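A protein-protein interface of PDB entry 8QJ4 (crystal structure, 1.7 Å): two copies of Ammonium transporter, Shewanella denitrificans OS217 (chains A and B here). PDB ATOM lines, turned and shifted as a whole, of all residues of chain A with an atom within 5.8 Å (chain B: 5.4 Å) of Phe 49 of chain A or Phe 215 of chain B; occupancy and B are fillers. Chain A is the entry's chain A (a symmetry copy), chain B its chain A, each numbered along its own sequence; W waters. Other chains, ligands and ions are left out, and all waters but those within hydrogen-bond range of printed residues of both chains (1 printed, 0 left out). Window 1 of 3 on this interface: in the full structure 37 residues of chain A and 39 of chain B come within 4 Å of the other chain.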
ATOM      1  N   LEU A  19      32.372  19.522  -0.024  1.00  0.00           N
ATOM      2  CA  LEU A  19      31.810  18.789   1.104  1.00  0.00           C
ATOM      3  C   LEU A  19      32.890  18.397   2.103  1.00  0.00           C
ATOM      4  O   LEU A  19      32.623  18.465   3.313  1.00  0.00           O
ATOM      5  CB  LEU A  19      31.045  17.564   0.645  1.00  0.00           C
ATOM      6  CG  LEU A  19      30.440  16.685   1.735  1.00  0.00           C
ATOM      7  CD1 LEU A  19      29.493  17.450   2.621  1.00  0.00           C
ATOM      8  CD2 LEU A  19      29.694  15.503   1.137  1.00  0.00           C
ATOM      9  N   GLN A  22      33.447  20.766   4.946  1.00  0.00           N
ATOM     10  CA  GLN A  22      32.578  20.660   6.116  1.00  0.00           C
ATOM     11  C   GLN A  22      33.156  19.713   7.180  1.00  0.00           C
ATOM     12  O   GLN A  22      33.119  20.040   8.370  1.00  0.00           O
ATOM     13  CB  GLN A  22      31.170  20.178   5.720  1.00  0.00           C
ATOM     14  CG  GLN A  22      30.622  20.897   4.458  1.00  0.00           C
ATOM     15  CD  GLN A  22      30.796  22.424   4.255  1.00  0.00           C
ATOM     16  OE1 GLN A  22      30.219  23.162   5.087  1.00  0.00           O
ATOM     17  NE2 GLN A  22      31.459  22.880   3.133  1.00  0.00           N
ATOM     18  N   LYS A  44      26.827  21.271  16.274  1.00  0.00           N
ATOM     19  CA  LYS A  44      26.617  22.503  15.501  1.00  0.00           C
ATOM     20  C   LYS A  44      27.003  22.280  14.038  1.00  0.00           C
ATOM     21  O   LYS A  44      26.288  22.739  13.122  1.00  0.00           O
ATOM     22  CB  LYS A  44      27.424  23.688  16.040  1.00  0.00           C
ATOM     23  CG  LYS A  44      26.934  24.292  17.352  1.00  0.00           C
ATOM     24  CD  LYS A  44      27.719  25.536  17.734  1.00  0.00           C
ATOM     25  CE  LYS A  44      29.168  25.244  18.018  1.00  0.00           C
ATOM     26  NZ  LYS A  44      30.020  26.442  18.230  1.00  0.00           N
ATOM     27  N   ASN A  45      28.131  21.587  13.817  1.00  0.00           N
ATOM     28  CA  ASN A  45      28.741  21.462  12.502  1.00  0.00           C
ATOM     29  C   ASN A  45      27.963  20.498  11.605  1.00  0.00           C
ATOM     30  O   ASN A  45      28.068  20.610  10.392  1.00  0.00           O
ATOM     31  CB  ASN A  45      30.232  21.116  12.614  1.00  0.00           C
ATOM     32  CG  ASN A  45      31.053  22.369  12.765  1.00  0.00           C
ATOM     33  OD1 ASN A  45      31.390  23.056  11.782  1.00  0.00           O
ATOM     34  ND2 ASN A  45      31.407  22.723  13.984  1.00  0.00           N
ATOM     35  N   VAL A  46      27.313  19.469  12.121  1.00  0.00           N
ATOM     36  CA  VAL A  46      26.436  18.646  11.299  1.00  0.00           C
ATOM     37  C   VAL A  46      25.047  19.291  11.122  1.00  0.00           C
ATOM     38  O   VAL A  46      24.488  19.239  10.023  1.00  0.00           O
ATOM     39  CB  VAL A  46      26.310  17.212  11.778  1.00  0.00           C
ATOM     40  CG1 VAL A  46      25.646  17.057  13.132  1.00  0.00           C
ATOM     41  CG2 VAL A  46      25.568  16.339  10.753  1.00  0.00           C
ATOM     42  N   SER A  47      24.539  19.933  12.182  1.00  0.00           N
ATOM     43  CA  SER A  47      23.211  20.553  12.106  1.00  0.00           C
ATOM     44  C   SER A  47      23.165  21.706  11.129  1.00  0.00           C
ATOM     45  O   SER A  47      22.169  21.856  10.396  1.00  0.00           O
ATOM     46  CB  SER A  47      22.771  20.984  13.490  1.00  0.00           C
ATOM     47  OG  SER A  47      22.702  19.862  14.353  1.00  0.00           O
ATOM     48  N   ASP A  48      24.184  22.595  11.134  1.00  0.00           N
ATOM     49  CA  ASP A  48      24.166  23.735  10.254  1.00  0.00           C
ATOM     50  C   ASP A  48      24.174  23.277   8.805  1.00  0.00           C
ATOM     51  O   ASP A  48      23.537  23.906   7.935  1.00  0.00           O
ATOM     52  CB  ASP A  48      25.202  24.822  10.594  1.00  0.00           C
ATOM     53  CG  ASP A  48      26.669  24.448  10.573  1.00  0.00           C
ATOM     54  OD1 ASP A  48      26.941  23.390  10.026  1.00  0.00           O
ATOM     55  OD2 ASP A  48      27.516  25.260  11.094  1.00  0.00           O
ATOM     56  N   PHE A  49      24.962  22.245   8.497  1.00  0.00           N
ATOM     57  CA  PHE A  49      25.027  21.695   7.145  1.00  0.00           C
ATOM     58  C   PHE A  49      23.642  21.238   6.665  1.00  0.00           C
ATOM     59  O   PHE A  49      23.198  21.618   5.586  1.00  0.00           O
ATOM     60  CB  PHE A  49      25.978  20.510   7.131  1.00  0.00           C
ATOM     61  CG  PHE A  49      26.030  19.858   5.773  1.00  0.00           C
ATOM     62  CD1 PHE A  49      26.621  20.483   4.707  1.00  0.00           C
ATOM     63  CD2 PHE A  49      25.578  18.564   5.639  1.00  0.00           C
ATOM     64  CE1 PHE A  49      26.630  19.903   3.449  1.00  0.00           C
ATOM     65  CE2 PHE A  49      25.663  17.948   4.404  1.00  0.00           C
ATOM     66  CZ  PHE A  49      26.134  18.644   3.324  1.00  0.00           C
ATOM     67  N   CYS A  50      22.938  20.506   7.510  1.00  0.00           N
ATOM     68  CA  CYS A  50      21.615  20.016   7.146  1.00  0.00           C
ATOM     69  C   CYS A  50      20.618  21.169   6.977  1.00  0.00           C
ATOM     70  O   CYS A  50      19.881  21.187   5.975  1.00  0.00           O
ATOM     71  CB  CYS A  50      21.073  18.989   8.100  1.00  0.00           C
ATOM     72  SG  CYS A  50      22.007  17.447   8.225  1.00  0.00           S
ATOM     73  N   VAL A  51      20.594  22.129   7.905  1.00  0.00           N
ATOM     74  CA  VAL A  51      19.703  23.274   7.844  1.00  0.00           C
ATOM     75  C   VAL A  51      19.947  24.118   6.588  1.00  0.00           C
ATOM     76  O   VAL A  51      19.006  24.505   5.862  1.00  0.00           O
ATOM     77  CB  VAL A  51      19.813  24.126   9.129  1.00  0.00           C
ATOM     78  CG1 VAL A  51      19.100  25.456   8.955  1.00  0.00           C
ATOM     79  CG2 VAL A  51      19.298  23.386  10.331  1.00  0.00           C
ATOM     80  N   CYS A  52      21.214  24.413   6.290  1.00  0.00           N
ATOM     81  CA  CYS A  52      21.576  25.222   5.148  1.00  0.00           C
ATOM     82  C   CYS A  52      21.187  24.534   3.847  1.00  0.00           C
ATOM     83  O   CYS A  52      20.660  25.172   2.900  1.00  0.00           O
ATOM     84  CB  CYS A  52      23.067  25.564   5.086  1.00  0.00           C
ATOM     85  SG  CYS A  52      23.537  26.764   6.346  1.00  0.00           S
ATOM     86  N   ALA A  53      21.461  23.229   3.754  1.00  0.00           N
ATOM     87  CA  ALA A  53      21.139  22.471   2.549  1.00  0.00           C
ATOM     88  C   ALA A  53      19.612  22.526   2.302  1.00  0.00           C
ATOM     89  O   ALA A  53      19.139  22.737   1.166  1.00  0.00           O
ATOM     90  CB  ALA A  53      21.594  21.029   2.683  1.00  0.00           C
ATOM     91  N   VAL A  54      18.821  22.244   3.349  1.00  0.00           N
ATOM     92  CA  VAL A  54      17.349  22.298   3.233  1.00  0.00           C
ATOM     93  C   VAL A  54      16.898  23.682   2.759  1.00  0.00           C
ATOM     94  O   VAL A  54      16.108  23.774   1.804  1.00  0.00           O
ATOM     95  CB  VAL A  54      16.661  21.916   4.566  1.00  0.00           C
ATOM     96  CG1 VAL A  54      15.155  22.234   4.535  1.00  0.00           C
ATOM     97  CG2 VAL A  54      16.912  20.443   4.869  1.00  0.00           C
ATOM     98  N   LEU A  96      24.942  24.984  -3.467  1.00  0.00           N
ATOM     99  CA  LEU A  96      24.392  24.551  -2.191  1.00  0.00           C
ATOM    100  C   LEU A  96      25.559  24.357  -1.216  1.00  0.00           C
ATOM    101  O   LEU A  96      25.477  24.812  -0.093  1.00  0.00           O
ATOM    102  CB  LEU A  96      23.580  23.249  -2.379  1.00  0.00           C
ATOM    103  CG  LEU A  96      23.003  22.613  -1.102  1.00  0.00           C
ATOM    104  CD1 LEU A  96      21.664  21.940  -1.360  1.00  0.00           C
ATOM    105  CD2 LEU A  96      23.941  21.588  -0.452  1.00  0.00           C
ATOM    106  N   MET A  97      26.661  23.723  -1.671  1.00  0.00           N
ATOM    107  CA  MET A  97      27.827  23.509  -0.801  1.00  0.00           C
ATOM    108  C   MET A  97      28.437  24.841  -0.415  1.00  0.00           C
ATOM    109  O   MET A  97      28.865  25.025   0.719  1.00  0.00           O
ATOM    110  CB  MET A  97      28.862  22.595  -1.463  1.00  0.00           C
ATOM    111  CG  MET A  97      28.368  21.214  -1.741  1.00  0.00           C
ATOM    112  SD  MET A  97      28.031  20.330  -0.227  1.00  0.00           S
ATOM    113  CE  MET A  97      27.384  18.806  -0.899  1.00  0.00           C
ATOM    114  N   CYS A 100      26.363  26.348   2.482  1.00  0.00           N
ATOM    115  CA  CYS A 100      26.728  25.624   3.704  1.00  0.00           C
ATOM    116  C   CYS A 100      28.067  26.091   4.263  1.00  0.00           C
ATOM    117  O   CYS A 100      28.153  26.261   5.475  1.00  0.00           O
ATOM    118  CB  CYS A 100      26.819  24.124   3.454  1.00  0.00           C
ATOM    119  SG  CYS A 100      25.231  23.372   2.980  1.00  0.00           S
ATOM    120  N   THR A 104      28.661  27.938   7.977  1.00  0.00           N
ATOM    121  CA  THR A 104      29.312  27.129   9.007  1.00  0.00           C
ATOM    122  C   THR A 104      30.552  27.851   9.544  1.00  0.00           C
ATOM    123  O   THR A 104      31.053  27.531  10.609  1.00  0.00           O
ATOM    124  CB  THR A 104      29.629  25.676   8.553  1.00  0.00           C
ATOM    125  OG1 THR A 104      29.692  24.885   9.734  1.00  0.00           O
ATOM    126  CG2 THR A 104      30.898  25.601   7.756  1.00  0.00           C
ATOM    127  N   GLY B 210      33.550  11.247  10.870  1.00  0.00           N
ATOM    128  CA  GLY B 210      33.243  10.014  10.191  1.00  0.00           C
ATOM    129  C   GLY B 210      31.981  10.065   9.341  1.00  0.00           C
ATOM    130  O   GLY B 210      31.953   9.501   8.231  1.00  0.00           O
ATOM    131  N   THR B 211      30.936  10.721   9.904  1.00  0.00           N
ATOM    132  CA  THR B 211      29.679  10.877   9.197  1.00  0.00           C
ATOM    133  C   THR B 211      29.905  11.705   7.928  1.00  0.00           C
ATOM    134  O   THR B 211      29.411  11.358   6.834  1.00  0.00           O
ATOM    135  CB  THR B 211      28.619  11.526  10.113  1.00  0.00           C
ATOM    136  OG1 THR B 211      28.481  10.698  11.255  1.00  0.00           O
ATOM    137  CG2 THR B 211      27.283  11.714   9.426  1.00  0.00           C
ATOM    138  N   PHE B 212      30.686  12.787   7.999  1.00  0.00           N
ATOM    139  CA  PHE B 212      30.971  13.560   6.794  1.00  0.00           C
ATOM    140  C   PHE B 212      31.780  12.749   5.754  1.00  0.00           C
ATOM    141  O   PHE B 212      31.556  12.875   4.549  1.00  0.00           O
ATOM    142  CB  PHE B 212      31.691  14.881   7.118  1.00  0.00           C
ATOM    143  CG  PHE B 212      30.751  15.968   7.528  1.00  0.00           C
ATOM    144  CD1 PHE B 212      29.863  16.474   6.597  1.00  0.00           C
ATOM    145  CD2 PHE B 212      30.752  16.496   8.789  1.00  0.00           C
ATOM    146  CE1 PHE B 212      29.005  17.522   6.951  1.00  0.00           C
ATOM    147  CE2 PHE B 212      29.926  17.548   9.119  1.00  0.00           C
ATOM    148  CZ  PHE B 212      29.050  18.062   8.189  1.00  0.00           C
ATOM    149  N   LEU B 213      32.764  11.938   6.206  1.00  0.00           N
ATOM    150  CA  LEU B 213      33.495  11.097   5.298  1.00  0.00           C
ATOM    151  C   LEU B 213      32.591  10.048   4.630  1.00  0.00           C
ATOM    152  O   LEU B 213      32.733   9.757   3.443  1.00  0.00           O
ATOM    153  CB  LEU B 213      34.693  10.419   5.979  1.00  0.00           C
ATOM    154  CG  LEU B 213      35.755  11.382   6.524  1.00  0.00           C
ATOM    155  CD1 LEU B 213      36.901  10.669   7.151  1.00  0.00           C
ATOM    156  CD2 LEU B 213      36.245  12.329   5.497  1.00  0.00           C
ATOM    157  N   LEU B 214      31.666   9.469   5.395  1.00  0.00           N
ATOM    158  CA  LEU B 214      30.703   8.547   4.826  1.00  0.00           C
ATOM    159  C   LEU B 214      29.845   9.241   3.747  1.00  0.00           C
ATOM    160  O   LEU B 214      29.574   8.635   2.713  1.00  0.00           O
ATOM    161  CB  LEU B 214      29.856   7.923   5.937  1.00  0.00           C
ATOM    162  CG  LEU B 214      30.587   6.883   6.775  1.00  0.00           C
ATOM    163  CD1 LEU B 214      29.865   6.582   8.066  1.00  0.00           C
ATOM    164  CD2 LEU B 214      30.726   5.587   5.993  1.00  0.00           C
ATOM    165  N   PHE B 215      29.373  10.431   4.072  1.00  0.00           N
ATOM    166  CA  PHE B 215      28.542  11.232   3.188  1.00  0.00           C
ATOM    167  C   PHE B 215      29.277  11.454   1.876  1.00  0.00           C
ATOM    168  O   PHE B 215      28.762  11.221   0.777  1.00  0.00           O
ATOM    169  CB  PHE B 215      28.156  12.519   3.867  1.00  0.00           C
ATOM    170  CG  PHE B 215      26.873  13.155   3.339  1.00  0.00           C
ATOM    171  CD1 PHE B 215      26.541  13.162   2.006  1.00  0.00           C
ATOM    172  CD2 PHE B 215      26.065  13.851   4.205  1.00  0.00           C
ATOM    173  CE1 PHE B 215      25.404  13.838   1.531  1.00  0.00           C
ATOM    174  CE2 PHE B 215      24.906  14.480   3.739  1.00  0.00           C
ATOM    175  CZ  PHE B 215      24.577  14.463   2.410  1.00  0.00           C
ATOM    176  N   LEU B 216      30.514  11.912   1.983  1.00  0.00           N
ATOM    177  CA  LEU B 216      31.342  12.188   0.819  1.00  0.00           C
ATOM    178  C   LEU B 216      31.492  10.934  -0.028  1.00  0.00           C
ATOM    179  O   LEU B 216      31.317  10.933  -1.251  1.00  0.00           O
ATOM    180  CB  LEU B 216      32.716  12.713   1.302  1.00  0.00           C
ATOM    181  CG  LEU B 216      33.817  12.713   0.267  1.00  0.00           C
ATOM    182  CD1 LEU B 216      33.437  13.628  -0.862  1.00  0.00           C
ATOM    183  CD2 LEU B 216      35.105  13.163   0.953  1.00  0.00           C
ATOM    184  N   GLY B 217      31.804   9.831   0.624  1.00  0.00           N
ATOM    185  CA  GLY B 217      31.993   8.605  -0.046  1.00  0.00           C
ATOM    186  C   GLY B 217      30.760   8.122  -0.777  1.00  0.00           C
ATOM    187  O   GLY B 217      30.880   7.427  -1.810  1.00  0.00           O
ATOM    188  N   TRP B 218      29.581   8.363  -0.173  1.00  0.00           N
ATOM    189  CA  TRP B 218      28.329   7.952  -0.731  1.00  0.00           C
ATOM    190  C   TRP B 218      28.115   8.579  -2.109  1.00  0.00           C
ATOM    191  O   TRP B 218      27.427   7.976  -2.955  1.00  0.00           O
ATOM    192  CB  TRP B 218      27.181   8.350   0.210  1.00  0.00           C
ATOM    193  CG  TRP B 218      26.303   7.212   0.513  1.00  0.00           C
ATOM    194  CD1 TRP B 218      25.446   6.594  -0.335  1.00  0.00           C
ATOM    195  CD2 TRP B 218      26.229   6.521   1.769  1.00  0.00           C
ATOM    196  NE1 TRP B 218      24.808   5.593   0.339  1.00  0.00           N
ATOM    197  CE2 TRP B 218      25.306   5.470   1.601  1.00  0.00           C
ATOM    198  CE3 TRP B 218      26.789   6.705   3.013  1.00  0.00           C
ATOM    199  CZ2 TRP B 218      24.933   4.630   2.628  1.00  0.00           C
ATOM    200  CZ3 TRP B 218      26.396   5.872   4.058  1.00  0.00           C
ATOM    201  CH2 TRP B 218      25.511   4.829   3.849  1.00  0.00           C
ATOM    202  N   PHE B 219      28.695   9.751  -2.373  1.00  0.00           N
ATOM    203  CA  PHE B 219      28.597  10.305  -3.727  1.00  0.00           C
ATOM    204  C   PHE B 219      29.270   9.405  -4.769  1.00  0.00           C
ATOM    205  O   PHE B 219      28.757   9.245  -5.897  1.00  0.00           O
ATOM    206  CB  PHE B 219      29.153  11.733  -3.791  1.00  0.00           C
ATOM    207  CG  PHE B 219      28.276  12.760  -3.149  1.00  0.00           C
ATOM    208  CD1 PHE B 219      27.113  13.202  -3.763  1.00  0.00           C
ATOM    209  CD2 PHE B 219      28.455  13.132  -1.852  1.00  0.00           C
ATOM    210  CE1 PHE B 219      26.277  14.150  -3.215  1.00  0.00           C
ATOM    211  CE2 PHE B 219      27.600  14.068  -1.250  1.00  0.00           C
ATOM    212  CZ  PHE B 219      26.552  14.641  -1.977  1.00  0.00           C
ATOM    213  N   THR B 240      21.343  12.298  -3.631  1.00  0.00           N
ATOM    214  CA  THR B 240      22.205  11.827  -2.533  1.00  0.00           C
ATOM    215  C   THR B 240      22.318  12.892  -1.449  1.00  0.00           C
ATOM    216  O   THR B 240      22.058  12.618  -0.266  1.00  0.00           O
ATOM    217  CB  THR B 240      23.593  11.398  -3.077  1.00  0.00           C
ATOM    218  OG1 THR B 240      23.421  10.398  -4.090  1.00  0.00           O
ATOM    219  CG2 THR B 240      24.514  10.923  -1.983  1.00  0.00           C
ATOM    220  N   ALA B 241      22.605  14.125  -1.843  1.00  0.00           N
ATOM    221  CA  ALA B 241      22.717  15.256  -0.931  1.00  0.00           C
ATOM    222  C   ALA B 241      21.422  15.479  -0.155  1.00  0.00           C
ATOM    223  O   ALA B 241      21.413  15.695   1.064  1.00  0.00           O
ATOM    224  CB  ALA B 241      23.086  16.489  -1.675  1.00  0.00           C
ATOM    225  N   GLY B 244      20.529  12.564   2.507  1.00  0.00           N
ATOM    226  CA  GLY B 244      21.282  12.739   3.728  1.00  0.00           C
ATOM    227  C   GLY B 244      20.880  13.942   4.551  1.00  0.00           C
ATOM    228  O   GLY B 244      20.728  13.833   5.778  1.00  0.00           O
ATOM    229  N   THR B 245      20.774  15.091   3.892  1.00  0.00           N
ATOM    230  CA  THR B 245      20.484  16.297   4.636  1.00  0.00           C
ATOM    231  C   THR B 245      19.080  16.255   5.203  1.00  0.00           C
ATOM    232  O   THR B 245      18.902  16.739   6.307  1.00  0.00           O
ATOM    233  CB  THR B 245      20.860  17.567   3.865  1.00  0.00           C
ATOM    234  OG1 THR B 245      20.114  17.514   2.669  1.00  0.00           O
ATOM    235  CG2 THR B 245      22.333  17.667   3.554  1.00  0.00           C
ATOM    236  N   VAL B 271      21.319  11.264   9.219  1.00  0.00           N
ATOM    237  CA  VAL B 271      22.001  11.549   7.959  1.00  0.00           C
ATOM    238  C   VAL B 271      22.332  10.242   7.270  1.00  0.00           C
ATOM    239  O   VAL B 271      22.019  10.025   6.099  1.00  0.00           O
ATOM    240  CB  VAL B 271      23.288  12.358   8.179  1.00  0.00           C
ATOM    241  CG1 VAL B 271      24.086  12.453   6.884  1.00  0.00           C
ATOM    242  CG2 VAL B 271      22.989  13.730   8.771  1.00  0.00           C
ATOM    243  N   LEU B 272      22.946   9.286   8.002  1.00  0.00           N
ATOM    244  CA  LEU B 272      23.361   8.033   7.375  1.00  0.00           C
ATOM    245  C   LEU B 272      22.144   7.238   6.877  1.00  0.00           C
ATOM    246  O   LEU B 272      22.168   6.651   5.819  1.00  0.00           O
ATOM    247  CB  LEU B 272      24.155   7.197   8.364  1.00  0.00           C
ATOM    248  CG  LEU B 272      25.472   7.831   8.856  1.00  0.00           C
ATOM    249  CD1 LEU B 272      26.186   6.910   9.826  1.00  0.00           C
ATOM    250  CD2 LEU B 272      26.349   8.208   7.676  1.00  0.00           C
ATOM    251  N   LEU B 275      20.864   8.614   3.647  1.00  0.00           N
ATOM    252  CA  LEU B 275      21.718   8.180   2.553  1.00  0.00           C
ATOM    253  C   LEU B 275      21.454   6.727   2.173  1.00  0.00           C
ATOM    254  O   LEU B 275      21.327   6.379   0.980  1.00  0.00           O
ATOM    255  CB  LEU B 275      23.177   8.396   2.943  1.00  0.00           C
ATOM    256  CG  LEU B 275      23.611   9.844   2.998  1.00  0.00           C
ATOM    257  CD1 LEU B 275      24.939   9.944   3.771  1.00  0.00           C
ATOM    258  CD2 LEU B 275      23.685  10.479   1.630  1.00  0.00           C
HETATM  259  O   HOH W   1      32.996  15.491   4.108  1.00  0.00           O
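The backbone carbonyl oxygen (O) of Thr 245 of chain B lies close to the side-chain sulfur (SG) of Cys 50 of chain A (3.7 Å).
The backbone carbonyl oxygen of Phe 49 of chain A sits close to the side-chain sulfur of Cys 100 of chain A.
The side-chain amide oxygen of Asn 45 of chain A lies within hydrogen-bond range of the side-chain hydroxyl of Thr 104 of chain A (3.2 Å).
The backbone carbonyl oxygen of Val 46 of chain A lies within hydrogen-bond range of the side-chain sulfur of Cys 50 of chain A, 3.5 Å away.
The backbone carbonyl oxygen of Ala 241 of chain B lies within hydrogen-bond range of the side-chain hydroxyl of Thr 245 of chain B (2.8 Å).
Among the printed residues, merely in contact across the chains: Leu 19 of chain A with Leu 216 of chain B, Leu 19 of chain A with Phe 219 of chain B, Gln 22 of chain A with Phe 212 of chain B, Asn 45 of chain A with Phe 212 of chain B, Phe 49 of chain A with Phe 212 of chain B, Phe 49 of chain A with Phe 215 of chain B, Phe 49 of chain A with Thr 245 of chain B, Cys 50 of chain A with Val 271 of chain B and Ala 53 of chain A with Thr 245 of chain B.
Of the printed residues of chain A, Phe 215 of chain B touches Phe 49 (3.6 Å).
Of the printed residues of chain A, Thr 245 of chain B touches Phe 49 (3.4 Å), Cys 50 (3.6 Å) and Ala 53 (3.6 Å).
Of the printed residues of chain A, Phe 212 of chain B touches Gln 22, Asn 45 and Phe 49.
Of the printed residues of chain B, Asn 45 of chain A touches Phe 212.
Of the printed residues of chain A, Phe 219 of chain B touches Leu 19 (3.5 Å).
Val 46 of chain A touches none of the printed residues of chain B.
Of the 17 printed residues of chain B, 6 touch a printed residue of chain A.
Printed residues of chain B that touch a printed residue of chain A: Phe 212, Phe 215, Leu 216, Phe 219, Thr 245 and Val 271.
Hydrophobic or aromatic side chains of chain B that line the printed part of chain A: Phe 212, Phe 215, Phe 219 and Val 271.
Along chain A the printed residues that touch a printed residue of chain B span positions 19 to 53.
Among the printed residues, no Asp or Glu carboxylate lies within 4 Å of a Lys or Arg side-chain nitrogen of the other chain.
No position is printed for both chains.
Of the 10 pairs that touch across the chains among the printed residues, none has its exchanged pair printed and touching as well.
Water W1 bridges O of Phe 212 of chain B (3.0 Å) and O of Leu 19 of chain A (3.1 Å).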
